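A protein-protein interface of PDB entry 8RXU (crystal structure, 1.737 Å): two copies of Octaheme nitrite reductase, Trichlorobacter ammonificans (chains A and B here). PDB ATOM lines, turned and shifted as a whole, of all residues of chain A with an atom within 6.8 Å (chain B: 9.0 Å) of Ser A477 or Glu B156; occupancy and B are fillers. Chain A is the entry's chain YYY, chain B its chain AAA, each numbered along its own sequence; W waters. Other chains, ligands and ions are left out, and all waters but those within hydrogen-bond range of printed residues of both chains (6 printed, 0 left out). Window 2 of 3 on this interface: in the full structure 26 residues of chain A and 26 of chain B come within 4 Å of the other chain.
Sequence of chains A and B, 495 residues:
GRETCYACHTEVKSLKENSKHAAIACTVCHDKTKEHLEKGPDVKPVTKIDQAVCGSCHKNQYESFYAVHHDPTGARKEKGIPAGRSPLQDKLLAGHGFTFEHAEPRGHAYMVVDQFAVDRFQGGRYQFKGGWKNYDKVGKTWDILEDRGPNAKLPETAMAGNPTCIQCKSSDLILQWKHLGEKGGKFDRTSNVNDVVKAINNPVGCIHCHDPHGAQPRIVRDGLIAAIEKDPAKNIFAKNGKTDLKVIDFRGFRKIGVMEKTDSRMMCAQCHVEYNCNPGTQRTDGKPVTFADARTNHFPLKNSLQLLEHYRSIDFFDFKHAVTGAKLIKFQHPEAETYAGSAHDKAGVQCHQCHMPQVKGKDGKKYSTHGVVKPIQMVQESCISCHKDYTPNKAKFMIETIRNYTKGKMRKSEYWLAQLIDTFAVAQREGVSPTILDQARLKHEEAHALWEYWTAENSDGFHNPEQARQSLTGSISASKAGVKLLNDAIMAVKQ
No position is printed for both chains.
Of the printed residues of chain B, Thr A473 touches Pro B155 (3.999 Å) and Glu B156 (3.4 Å).
Of chain B, only Glu B156 (3.4 Å) comes within 4 Å of Ile A476.
Of the printed residues of chain A, Pro B155 touches Arg A469 (3.1 Å) and Thr A473 (3.999 Å).
Glu B156 touches just these residues of chain A: Arg A469 (3.4 Å), Thr A473 (3.4 Å), Ile A476 (3.4 Å), Ser A477 (2.9 Å) and Lys A480 (2.5 Å).
Of the printed residues of chain A, Thr B157 touches Arg A469.
The nearest residue of chain A that does not touch Glu B156 is Lys A409 (4.6 Å).
N of Asp B119 lies within hydrogen-bond range of OE1 of Glu B101, 2.9 Å away.
The guanidinium group (NE) of Arg B76 is in salt-bridge range of the side-chain carboxylate (OE2) of Glu B101, 2.9 Å away.
Of the 19 printed residues of chain B, 10 touch a printed residue of chain A.
Hydrophobic or aromatic side chains of chain B within 4 Å of the printed part of chain A: Phe B100, Leu B154 and Pro B155.
Printed residues of chain A that touch a printed residue of chain B: Tyr A405, Lys A409, Lys A412, Arg A469, Thr A473, Ile A476, Ser A477 and Lys A480.
Hydrophobic or aromatic side chains of chain A that line the printed part of chain B: Tyr A405 and Ile A476.
Water W6 lies within hydrogen-bond range of the side-chain carboxylate (OD1) of Asp B119 and the side-chain hydroxyl (OH) of Tyr A405.
Water W3 lies within hydrogen-bond range of NZ of Lys A409 (3.3 Å) and O of Phe B100 (3.5 Å).
Among the printed residues, pairs that only touch across the chains: Ile A476 with Glu B156 (3.4 Å), Arg A469 with Leu B154 (3.4 Å), Thr A473 with Glu B156 (3.4 Å), Lys A480 with Phe B100 (3.5 Å), Tyr A405 with Arg B76 (3.5 Å), Arg A469 with Thr B157 (3.6 Å), Tyr A405 with Glu B101 (3.7 Å) and Thr A473 with Pro B155 (3.999 Å).
NZ of Lys A409 sits at hydrogen-bond distance from O of Phe B100, 3.0 Å away.
OE2 of Glu B156 lies within hydrogen-bond range of OG of Ser A477, at 2.9 Å.
NH2 of Arg A469 lies within hydrogen-bond range of O of Glu B156, 3.4 Å away.
The side-chain carboxylate (OD1) of Asp B90 is in salt-bridge range of the side-chain amino group (NZ) of Lys A412 (2.9 Å).
The side-chain carboxylate (OE1) of Glu B156 is in salt-bridge range of the side-chain amino group (NZ) of Lys A480 (2.5 Å).
NH2 of Arg A469 lies within salt-bridge range of OD2 of Asp B119.
The guanidinium group (NH2) of Arg A469 lies within hydrogen-bond range of the backbone carbonyl oxygen (O) of Pro B155.
NZ of Lys A412 sits at hydrogen-bond distance from O of Thr B99.
The side-chain carboxylate (OD2) of Asp B119 lies within hydrogen-bond range of the side-chain hydroxyl (OH) of Tyr A405, 2.6 Å away.
OD2 of Asp B119 lies within salt-bridge range of NZ of Lys A409, 2.6 Å away.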
ATOM      1  N   TYR A 405       1.561  22.318  27.262  1.00  0.00           N
ATOM      2  CA  TYR A 405       0.552  22.977  26.395  1.00  0.00           C
ATOM      3  C   TYR A 405      -0.355  21.863  25.845  1.00  0.00           C
ATOM      4  O   TYR A 405      -1.585  21.963  25.975  1.00  0.00           O
ATOM      5  CB  TYR A 405       1.175  23.814  25.291  1.00  0.00           C
ATOM      6  CG  TYR A 405       0.114  24.408  24.396  1.00  0.00           C
ATOM      7  CD1 TYR A 405      -0.570  25.555  24.769  1.00  0.00           C
ATOM      8  CD2 TYR A 405      -0.306  23.736  23.262  1.00  0.00           C
ATOM      9  CE1 TYR A 405      -1.550  26.127  23.966  1.00  0.00           C
ATOM     10  CE2 TYR A 405      -1.264  24.301  22.434  1.00  0.00           C
ATOM     11  CZ  TYR A 405      -1.910  25.468  22.794  1.00  0.00           C
ATOM     12  OH  TYR A 405      -2.925  25.980  22.024  1.00  0.00           O
ATOM     13  N   LYS A 409      -4.552  20.701  26.638  1.00  0.00           N
ATOM     14  CA  LYS A 409      -5.666  20.457  25.665  1.00  0.00           C
ATOM     15  C   LYS A 409      -6.178  19.032  25.788  1.00  0.00           C
ATOM     16  O   LYS A 409      -7.398  18.872  25.543  1.00  0.00           O
ATOM     17  CB  LYS A 409      -5.260  20.789  24.228  1.00  0.00           C
ATOM     18  CG  LYS A 409      -4.755  22.191  24.054  1.00  0.00           C
ATOM     19  CD  LYS A 409      -5.756  23.222  24.412  1.00  0.00           C
ATOM     20  CE  LYS A 409      -5.074  24.543  24.604  1.00  0.00           C
ATOM     21  NZ  LYS A 409      -5.964  25.688  24.430  1.00  0.00           N
ATOM     22  N   LYS A 412      -8.548  18.969  28.783  1.00  0.00           N
ATOM     23  CA  LYS A 412      -9.830  19.657  28.420  1.00  0.00           C
ATOM     24  C   LYS A 412     -10.644  18.768  27.489  1.00  0.00           C
ATOM     25  O   LYS A 412     -11.873  18.692  27.626  1.00  0.00           O
ATOM     26  CB  LYS A 412      -9.562  21.002  27.744  1.00  0.00           C
ATOM     27  CG  LYS A 412     -10.698  22.023  27.758  1.00  0.00           C
ATOM     28  CD  LYS A 412     -10.272  23.367  27.084  1.00  0.00           C
ATOM     29  CE  LYS A 412      -9.021  23.974  27.703  1.00  0.00           C
ATOM     30  NZ  LYS A 412      -9.224  24.262  29.147  1.00  0.00           N
ATOM     31  N   TRP A 416     -14.459  17.481  28.303  1.00  0.00           N
ATOM     32  CA  TRP A 416     -15.587  17.519  27.320  1.00  0.00           C
ATOM     33  C   TRP A 416     -16.142  16.136  26.958  1.00  0.00           C
ATOM     34  O   TRP A 416     -17.429  16.037  26.709  1.00  0.00           O
ATOM     35  CB  TRP A 416     -15.160  18.311  26.097  1.00  0.00           C
ATOM     36  CG  TRP A 416     -15.311  19.749  26.396  1.00  0.00           C
ATOM     37  CD1 TRP A 416     -14.357  20.617  26.821  1.00  0.00           C
ATOM     38  CD2 TRP A 416     -16.559  20.450  26.470  1.00  0.00           C
ATOM     39  NE1 TRP A 416     -14.920  21.819  27.143  1.00  0.00           N
ATOM     40  CE2 TRP A 416     -16.276  21.747  26.945  1.00  0.00           C
ATOM     41  CE3 TRP A 416     -17.885  20.070  26.263  1.00  0.00           C
ATOM     42  CZ2 TRP A 416     -17.267  22.717  27.105  1.00  0.00           C
ATOM     43  CZ3 TRP A 416     -18.863  21.025  26.416  1.00  0.00           C
ATOM     44  CH2 TRP A 416     -18.568  22.318  26.854  1.00  0.00           C
ATOM     45  N   LYS A 443     -20.620  12.121  17.102  1.00  0.00           N
ATOM     46  CA  LYS A 443     -19.851  13.208  17.774  1.00  0.00           C
ATOM     47  C   LYS A 443     -18.926  12.592  18.823  1.00  0.00           C
ATOM     48  O   LYS A 443     -17.739  12.988  18.841  1.00  0.00           O
ATOM     49  CB  LYS A 443     -20.779  14.292  18.314  1.00  0.00           C
ATOM     50  CG  LYS A 443     -21.286  15.271  17.260  1.00  0.00           C
ATOM     51  CD  LYS A 443     -20.242  15.831  16.299  1.00  0.00           C
ATOM     52  CE  LYS A 443     -20.855  16.680  15.205  1.00  0.00           C
ATOM     53  NZ  LYS A 443     -19.811  17.247  14.315  1.00  0.00           N
ATOM     54  N   GLU A 446     -16.165  10.940  16.870  1.00  0.00           N
ATOM     55  CA  GLU A 446     -15.187  11.922  16.350  1.00  0.00           C
ATOM     56  C   GLU A 446     -14.314  12.437  17.497  1.00  0.00           C
ATOM     57  O   GLU A 446     -13.093  12.600  17.292  1.00  0.00           O
ATOM     58  CB  GLU A 446     -15.905  13.118  15.724  1.00  0.00           C
ATOM     59  CG  GLU A 446     -14.971  14.280  15.396  1.00  0.00           C
ATOM     60  CD  GLU A 446     -15.221  15.036  14.092  1.00  0.00           C
ATOM     61  OE1 GLU A 446     -15.868  14.441  13.145  1.00  0.00           O
ATOM     62  OE2 GLU A 446     -14.760  16.205  14.011  1.00  0.00           O
ATOM     63  N   ALA A 447     -14.943  12.808  18.608  1.00  0.00           N
ATOM     64  CA  ALA A 447     -14.248  13.477  19.725  1.00  0.00           C
ATOM     65  C   ALA A 447     -13.284  12.447  20.310  1.00  0.00           C
ATOM     66  O   ALA A 447     -12.104  12.808  20.613  1.00  0.00           O
ATOM     67  CB  ALA A 447     -15.246  13.933  20.747  1.00  0.00           C
ATOM     68  N   ARG A 469      -2.309  19.707  18.564  1.00  0.00           N
ATOM     69  CA  ARG A 469      -3.205  20.846  18.828  1.00  0.00           C
ATOM     70  C   ARG A 469      -4.420  20.756  17.884  1.00  0.00           C
ATOM     71  O   ARG A 469      -5.553  21.008  18.394  1.00  0.00           O
ATOM     72  CB  ARG A 469      -2.527  22.208  18.793  1.00  0.00           C
ATOM     73  CG  ARG A 469      -3.469  23.295  19.298  1.00  0.00           C
ATOM     74  CD  ARG A 469      -3.110  24.714  18.911  1.00  0.00           C
ATOM     75  NE  ARG A 469      -3.948  25.628  19.660  1.00  0.00           N
ATOM     76  CZ  ARG A 469      -5.224  25.874  19.346  1.00  0.00           C
ATOM     77  NH1 ARG A 469      -5.744  25.291  18.281  1.00  0.00           N
ATOM     78  NH2 ARG A 469      -5.945  26.695  20.087  1.00  0.00           N
ATOM     79  N   LEU A 472      -6.613  17.549  19.178  1.00  0.00           N
ATOM     80  CA  LEU A 472      -7.291  17.691  20.501  1.00  0.00           C
ATOM     81  C   LEU A 472      -8.345  18.808  20.553  1.00  0.00           C
ATOM     82  O   LEU A 472      -9.366  18.587  21.292  1.00  0.00           O
ATOM     83  CB  LEU A 472      -6.214  17.951  21.551  1.00  0.00           C
ATOM     84  CG  LEU A 472      -5.272  16.786  21.757  1.00  0.00           C
ATOM     85  CD1 LEU A 472      -3.991  17.271  22.454  1.00  0.00           C
ATOM     86  CD2 LEU A 472      -5.967  15.679  22.519  1.00  0.00           C
ATOM     87  N   THR A 473      -8.145  19.939  19.853  1.00  0.00           N
ATOM     88  CA  THR A 473      -9.120  21.055  19.664  1.00  0.00           C
ATOM     89  C   THR A 473     -10.308  20.581  18.839  1.00  0.00           C
ATOM     90  O   THR A 473     -11.472  20.959  19.252  1.00  0.00           O
ATOM     91  CB  THR A 473      -8.505  22.350  19.116  1.00  0.00           C
ATOM     92  OG1 THR A 473      -7.850  22.178  17.839  1.00  0.00           O
ATOM     93  CG2 THR A 473      -7.583  22.939  20.165  1.00  0.00           C
ATOM     94  N   GLY A 474     -10.009  19.798  17.799  1.00  0.00           N
ATOM     95  CA  GLY A 474     -10.928  18.921  17.041  1.00  0.00           C
ATOM     96  C   GLY A 474     -11.846  18.137  17.982  1.00  0.00           C
ATOM     97  O   GLY A 474     -13.077  18.116  17.726  1.00  0.00           O
ATOM     98  N   SER A 475     -11.290  17.445  18.976  1.00  0.00           N
ATOM     99  CA  SER A 475     -11.997  16.600  19.973  1.00  0.00           C
ATOM    100  C   SER A 475     -12.912  17.490  20.829  1.00  0.00           C
ATOM    101  O   SER A 475     -14.102  17.167  21.022  1.00  0.00           O
ATOM    102  CB  SER A 475     -10.997  15.824  20.829  1.00  0.00           C
ATOM    103  OG  SER A 475     -11.646  14.958  21.734  1.00  0.00           O
ATOM    104  N   ILE A 476     -12.347  18.554  21.406  1.00  0.00           N
ATOM    105  CA  ILE A 476     -13.091  19.558  22.220  1.00  0.00           C
ATOM    106  C   ILE A 476     -14.265  20.050  21.386  1.00  0.00           C
ATOM    107  O   ILE A 476     -15.387  19.975  21.902  1.00  0.00           O
ATOM    108  CB  ILE A 476     -12.211  20.728  22.664  1.00  0.00           C
ATOM    109  CG1 ILE A 476     -11.128  20.232  23.617  1.00  0.00           C
ATOM    110  CG2 ILE A 476     -13.056  21.827  23.322  1.00  0.00           C
ATOM    111  CD1 ILE A 476      -9.946  21.119  23.698  1.00  0.00           C
ATOM    112  N   SER A 477     -13.991  20.467  20.155  1.00  0.00           N
ATOM    113  CA  SER A 477     -15.014  20.986  19.194  1.00  0.00           C
ATOM    114  C   SER A 477     -16.131  19.952  18.988  1.00  0.00           C
ATOM    115  O   SER A 477     -17.354  20.370  19.090  1.00  0.00           O
ATOM    116  CB  SER A 477     -14.394  21.402  17.908  1.00  0.00           C
ATOM    117  OG  SER A 477     -13.919  22.720  18.016  1.00  0.00           O
ATOM    118  N   ALA A 478     -15.798  18.677  18.780  1.00  0.00           N
ATOM    119  CA  ALA A 478     -16.811  17.614  18.500  1.00  0.00           C
ATOM    120  C   ALA A 478     -17.669  17.378  19.741  1.00  0.00           C
ATOM    121  O   ALA A 478     -18.847  17.146  19.600  1.00  0.00           O
ATOM    122  CB  ALA A 478     -16.178  16.335  18.013  1.00  0.00           C
ATOM    123  N   SER A 479     -17.107  17.535  20.941  1.00  0.00           N
ATOM    124  CA  SER A 479     -17.803  17.184  22.194  1.00  0.00           C
ATOM    125  C   SER A 479     -18.813  18.296  22.557  1.00  0.00           C
ATOM    126  O   SER A 479     -19.957  17.983  22.906  1.00  0.00           O
ATOM    127  CB  SER A 479     -16.774  16.914  23.273  1.00  0.00           C
ATOM    128  OG  SER A 479     -16.159  15.646  23.093  1.00  0.00           O
ATOM    129  N   LYS A 480     -18.411  19.565  22.431  1.00  0.00           N
ATOM    130  CA  LYS A 480     -19.248  20.782  22.654  1.00  0.00           C
ATOM    131  C   LYS A 480     -20.457  20.751  21.693  1.00  0.00           C
ATOM    132  O   LYS A 480     -21.616  20.836  22.163  1.00  0.00           O
ATOM    133  CB  LYS A 480     -18.392  22.030  22.414  1.00  0.00           C
ATOM    134  CG  LYS A 480     -17.344  22.341  23.485  1.00  0.00           C
ATOM    135  CD  LYS A 480     -16.849  23.783  23.434  1.00  0.00           C
ATOM    136  CE  LYS A 480     -15.606  24.037  24.269  1.00  0.00           C
ATOM    137  NZ  LYS A 480     -14.979  25.315  23.886  1.00  0.00           N
ATOM    138  N   ALA A 481     -20.212  20.543  20.408  1.00  0.00           N
ATOM    139  CA  ALA A 481     -21.264  20.352  19.372  1.00  0.00           C
ATOM    140  C   ALA A 481     -22.169  19.181  19.773  1.00  0.00           C
ATOM    141  O   ALA A 481     -23.400  19.310  19.640  1.00  0.00           O
ATOM    142  CB  ALA A 481     -20.643  20.123  18.019  1.00  0.00           C
ATOM    143  N   GLY A 482     -21.572  18.083  20.246  1.00  0.00           N
ATOM    144  CA  GLY A 482     -22.276  16.875  20.711  1.00  0.00           C
ATOM    145  C   GLY A 482     -23.111  17.134  21.948  1.00  0.00           C
ATOM    146  O   GLY A 482     -24.228  16.595  22.004  1.00  0.00           O
ATOM    147  N   ARG B  76       3.931  27.557  29.986  1.00  0.00           N
ATOM    148  CA  ARG B  76       2.606  27.457  29.345  1.00  0.00           C
ATOM    149  C   ARG B  76       1.784  26.412  30.106  1.00  0.00           C
ATOM    150  O   ARG B  76       1.048  25.644  29.470  1.00  0.00           O
ATOM    151  CB  ARG B  76       2.727  27.196  27.841  1.00  0.00           C
ATOM    152  CG  ARG B  76       1.462  27.573  27.095  1.00  0.00           C
ATOM    153  CD  ARG B  76       1.543  28.798  26.208  1.00  0.00           C
ATOM    154  NE  ARG B  76       0.322  28.928  25.420  1.00  0.00           N
ATOM    155  CZ  ARG B  76       0.240  29.608  24.275  1.00  0.00           C
ATOM    156  NH1 ARG B  76       1.278  30.274  23.805  1.00  0.00           N
ATOM    157  NH2 ARG B  76      -0.908  29.655  23.620  1.00  0.00           N
ATOM    158  N   ASP B  90     -12.630  24.112  34.142  1.00  0.00           N
ATOM    159  CA  ASP B  90     -13.440  23.987  32.917  1.00  0.00           C
ATOM    160  C   ASP B  90     -14.913  23.932  33.330  1.00  0.00           C
ATOM    161  O   ASP B  90     -15.720  24.637  32.638  1.00  0.00           O
ATOM    162  CB  ASP B  90     -12.940  22.846  32.038  1.00  0.00           C
ATOM    163  CG  ASP B  90     -11.746  23.301  31.198  1.00  0.00           C
ATOM    164  OD1 ASP B  90     -11.955  24.071  30.211  1.00  0.00           O
ATOM    165  OD2 ASP B  90     -10.581  23.051  31.678  1.00  0.00           O
ATOM    166  N   GLY B  97     -14.372  33.000  28.954  1.00  0.00           N
ATOM    167  CA  GLY B  97     -13.206  32.899  28.047  1.00  0.00           C
ATOM    168  C   GLY B  97     -11.983  32.225  28.668  1.00  0.00           C
ATOM    169  O   GLY B  97     -11.190  31.722  27.914  1.00  0.00           O
ATOM    170  N   THR B  99     -11.772  29.361  29.949  1.00  0.00           N
ATOM    171  CA  THR B  99     -11.876  27.919  29.602  1.00  0.00           C
ATOM    172  C   THR B  99     -11.084  27.649  28.307  1.00  0.00           C
ATOM    173  O   THR B  99     -10.703  26.505  28.123  1.00  0.00           O
ATOM    174  CB  THR B  99     -13.350  27.498  29.619  1.00  0.00           C
ATOM    175  OG1 THR B  99     -13.966  27.957  28.412  1.00  0.00           O
ATOM    176  CG2 THR B  99     -14.034  28.057  30.847  1.00  0.00           C
ATOM    177  N   PHE B 100     -10.723  28.663  27.514  1.00  0.00           N
ATOM    178  CA  PHE B 100     -10.038  28.471  26.205  1.00  0.00           C
ATOM    179  C   PHE B 100      -8.543  28.327  26.485  1.00  0.00           C
ATOM    180  O   PHE B 100      -7.910  27.535  25.805  1.00  0.00           O
ATOM    181  CB  PHE B 100     -10.390  29.541  25.191  1.00  0.00           C
ATOM    182  CG  PHE B 100     -11.776  29.343  24.641  1.00  0.00           C
ATOM    183  CD1 PHE B 100     -12.860  29.940  25.248  1.00  0.00           C
ATOM    184  CD2 PHE B 100     -11.983  28.500  23.560  1.00  0.00           C
ATOM    185  CE1 PHE B 100     -14.138  29.741  24.755  1.00  0.00           C
ATOM    186  CE2 PHE B 100     -13.273  28.278  23.088  1.00  0.00           C
ATOM    187  CZ  PHE B 100     -14.333  28.925  23.663  1.00  0.00           C
ATOM    188  N   GLU B 101      -8.115  28.866  27.610  1.00  0.00           N
ATOM    189  CA  GLU B 101      -6.707  28.794  28.059  1.00  0.00           C
ATOM    190  C   GLU B 101      -6.420  29.840  29.135  1.00  0.00           C
ATOM    191  O   GLU B 101      -6.771  31.028  28.991  1.00  0.00           O
ATOM    192  CB  GLU B 101      -5.714  29.000  26.922  1.00  0.00           C
ATOM    193  CG  GLU B 101      -4.298  28.946  27.457  1.00  0.00           C
ATOM    194  CD  GLU B 101      -3.167  28.889  26.450  1.00  0.00           C
ATOM    195  OE1 GLU B 101      -3.350  29.393  25.304  1.00  0.00           O
ATOM    196  OE2 GLU B 101      -2.107  28.373  26.848  1.00  0.00           O
ATOM    197  N   VAL B 118      -1.737  34.003  23.811  1.00  0.00           N
ATOM    198  CA  VAL B 118      -2.609  33.077  24.568  1.00  0.00           C
ATOM    199  C   VAL B 118      -3.875  32.877  23.720  1.00  0.00           C
ATOM    200  O   VAL B 118      -4.294  33.868  23.031  1.00  0.00           O
ATOM    201  CB  VAL B 118      -2.915  33.537  26.010  1.00  0.00           C
ATOM    202  CG1 VAL B 118      -3.973  34.630  26.047  1.00  0.00           C
ATOM    203  CG2 VAL B 118      -3.298  32.331  26.842  1.00  0.00           C
ATOM    204  N   ASP B 119      -4.404  31.656  23.780  1.00  0.00           N
ATOM    205  CA  ASP B 119      -5.529  31.141  22.944  1.00  0.00           C
ATOM    206  C   ASP B 119      -6.758  32.020  23.195  1.00  0.00           C
ATOM    207  O   ASP B 119      -7.614  32.055  22.273  1.00  0.00           O
ATOM    208  CB  ASP B 119      -5.810  29.650  23.178  1.00  0.00           C
ATOM    209  CG  ASP B 119      -4.778  28.669  22.618  1.00  0.00           C
ATOM    210  OD1 ASP B 119      -3.862  29.089  21.897  1.00  0.00           O
ATOM    211  OD2 ASP B 119      -4.915  27.469  22.878  1.00  0.00           O
ATOM    212  N   ARG B 120      -6.870  32.664  24.377  1.00  0.00           N
ATOM    213  CA  ARG B 120      -8.065  33.457  24.782  1.00  0.00           C
ATOM    214  C   ARG B 120      -7.963  34.919  24.300  1.00  0.00           C
ATOM    215  O   ARG B 120      -8.958  35.659  24.537  1.00  0.00           O
ATOM    216  CB  ARG B 120      -8.364  33.410  26.294  1.00  0.00           C
ATOM    217  CG  ARG B 120      -7.286  33.995  27.204  1.00  0.00           C
ATOM    218  CD  ARG B 120      -7.849  34.050  28.620  1.00  0.00           C
ATOM    219  NE  ARG B 120      -7.031  34.885  29.477  1.00  0.00           N
ATOM    220  CZ  ARG B 120      -5.862  34.544  29.991  1.00  0.00           C
ATOM    221  NH1 ARG B 120      -5.352  33.343  29.768  1.00  0.00           N
ATOM    222  NH2 ARG B 120      -5.208  35.412  30.748  1.00  0.00           N
ATOM    223  N   PHE B 121      -6.846  35.368  23.692  1.00  0.00           N
ATOM    224  CA  PHE B 121      -6.615  36.788  23.332  1.00  0.00           C
ATOM    225  C   PHE B 121      -7.357  37.168  22.017  1.00  0.00           C
ATOM    226  O   PHE B 121      -8.424  37.791  22.156  1.00  0.00           O
ATOM    227  CB  PHE B 121      -5.124  37.153  23.377  1.00  0.00           C
ATOM    228  CG  PHE B 121      -4.804  38.610  23.141  1.00  0.00           C
ATOM    229  CD1 PHE B 121      -4.873  39.557  24.158  1.00  0.00           C
ATOM    230  CD2 PHE B 121      -4.503  39.078  21.866  1.00  0.00           C
ATOM    231  CE1 PHE B 121      -4.566  40.891  23.909  1.00  0.00           C
ATOM    232  CE2 PHE B 121      -4.219  40.411  21.620  1.00  0.00           C
ATOM    233  CZ  PHE B 121      -4.276  41.322  22.638  1.00  0.00           C
ATOM    234  N   GLY B 123      -8.074  35.061  18.836  1.00  0.00           N
ATOM    235  CA  GLY B 123      -8.386  33.914  17.952  1.00  0.00           C
ATOM    236  C   GLY B 123      -7.160  33.170  17.408  1.00  0.00           C
ATOM    237  O   GLY B 123      -7.214  32.554  16.288  1.00  0.00           O
ATOM    238  N   GLY B 124      -6.059  33.195  18.152  1.00  0.00           N
ATOM    239  CA  GLY B 124      -4.785  32.578  17.754  1.00  0.00           C
ATOM    240  C   GLY B 124      -4.086  33.339  16.655  1.00  0.00           C
ATOM    241  O   GLY B 124      -3.236  32.737  16.013  1.00  0.00           O
ATOM    242  N   LYS B 153      -7.985  31.951  11.315  1.00  0.00           N
ATOM    243  CA  LYS B 153      -8.756  31.350  12.425  1.00  0.00           C
ATOM    244  C   LYS B 153      -7.815  30.369  13.130  1.00  0.00           C
ATOM    245  O   LYS B 153      -6.852  29.908  12.490  1.00  0.00           O
ATOM    246  CB  LYS B 153     -10.015  30.656  11.889  1.00  0.00           C
ATOM    247  CG  LYS B 153     -11.320  31.455  11.908  1.00  0.00           C
ATOM    248  CD  LYS B 153     -11.637  32.225  10.629  1.00  0.00           C
ATOM    249  CE  LYS B 153     -11.509  33.727  10.794  1.00  0.00           C
ATOM    250  NZ  LYS B 153     -12.489  34.284  11.758  1.00  0.00           N
ATOM    251  N   LEU B 154      -8.006  30.116  14.428  1.00  0.00           N
ATOM    252  CA  LEU B 154      -7.432  28.905  15.068  1.00  0.00           C
ATOM    253  C   LEU B 154      -8.525  28.315  15.946  1.00  0.00           C
ATOM    254  O   LEU B 154      -9.074  29.032  16.774  1.00  0.00           O
ATOM    255  CB  LEU B 154      -6.117  29.220  15.803  1.00  0.00           C
ATOM    256  CG  LEU B 154      -4.862  28.577  15.195  1.00  0.00           C
ATOM    257  CD1 LEU B 154      -4.774  27.112  15.540  1.00  0.00           C
ATOM    258  CD2 LEU B 154      -4.799  28.745  13.677  1.00  0.00           C
ATOM    259  N   PRO B 155      -8.871  27.015  15.777  1.00  0.00           N
ATOM    260  CA  PRO B 155      -9.957  26.377  16.517  1.00  0.00           C
ATOM    261  C   PRO B 155      -9.780  26.439  18.046  1.00  0.00           C
ATOM    262  O   PRO B 155      -8.670  26.556  18.552  1.00  0.00           O
ATOM    263  CB  PRO B 155     -10.009  24.949  15.928  1.00  0.00           C
ATOM    264  CG  PRO B 155      -9.424  25.109  14.540  1.00  0.00           C
ATOM    265  CD  PRO B 155      -8.296  26.094  14.771  1.00  0.00           C
ATOM    266  N   GLU B 156     -10.909  26.524  18.741  1.00  0.00           N
ATOM    267  CA  GLU B 156     -10.988  26.582  20.227  1.00  0.00           C
ATOM    268  C   GLU B 156     -10.017  27.656  20.735  1.00  0.00           C
ATOM    269  O   GLU B 156      -9.027  27.340  21.453  1.00  0.00           O
ATOM    270  CB  GLU B 156     -10.734  25.220  20.874  1.00  0.00           C
ATOM    271  CG  GLU B 156     -11.746  24.150  20.517  1.00  0.00           C
ATOM    272  CD  GLU B 156     -13.083  24.412  21.183  1.00  0.00           C
ATOM    273  OE1 GLU B 156     -13.113  25.098  22.253  1.00  0.00           O
ATOM    274  OE2 GLU B 156     -14.078  23.878  20.689  1.00  0.00           O
ATOM    275  N   THR B 157     -10.318  28.888  20.357  1.00  0.00           N
ATOM    276  CA  THR B 157      -9.697  30.150  20.829  1.00  0.00           C
ATOM    277  C   THR B 157     -10.821  31.123  21.185  1.00  0.00           C
ATOM    278  O   THR B 157     -12.016  30.790  20.925  1.00  0.00           O
ATOM    279  CB  THR B 157      -8.766  30.710  19.755  1.00  0.00           C
ATOM    280  OG1 THR B 157      -9.532  30.988  18.578  1.00  0.00           O
ATOM    281  CG2 THR B 157      -7.612  29.780  19.461  1.00  0.00           C
ATOM    282  N   ALA B 158     -10.470  32.259  21.789  1.00  0.00           N
ATOM    283  CA  ALA B 158     -11.413  33.323  22.186  1.00  0.00           C
ATOM    284  C   ALA B 158     -10.842  34.696  21.826  1.00  0.00           C
ATOM    285  O   ALA B 158      -9.633  34.809  21.409  1.00  0.00           O
ATOM    286  CB  ALA B 158     -11.775  33.225  23.657  1.00  0.00           C
ATOM    287  N   MET B 159     -11.714  35.690  21.912  1.00  0.00           N
ATOM    288  CA  MET B 159     -11.419  37.078  21.496  1.00  0.00           C
ATOM    289  C   MET B 159     -11.558  38.004  22.711  1.00  0.00           C
ATOM    290  O   MET B 159     -12.265  38.999  22.605  1.00  0.00           O
ATOM    291  CB  MET B 159     -12.365  37.442  20.357  1.00  0.00           C
ATOM    292  CG  MET B 159     -12.147  36.568  19.123  1.00  0.00           C
ATOM    293  SD  MET B 159     -10.690  37.060  18.204  1.00  0.00           S
ATOM    294  CE  MET B 159     -11.292  38.528  17.371  1.00  0.00           C
HETATM  295  O   HOH W   1     -13.764  26.543  26.259  1.00  0.00           O
HETATM  296  O   HOH W   2     -13.815  24.049  28.386  1.00  0.00           O
HETATM  297  O   HOH W   3      -5.714  25.619  27.675  1.00  0.00           O
HETATM  298  O   HOH W   4      -8.354  27.048  30.305  1.00  0.00           O
HETATM  299  O   HOH W   5      -8.465  25.713  23.588  1.00  0.00           O
HETATM  300  O   HOH W   6      -1.552  28.476  20.125  1.00  0.00           O
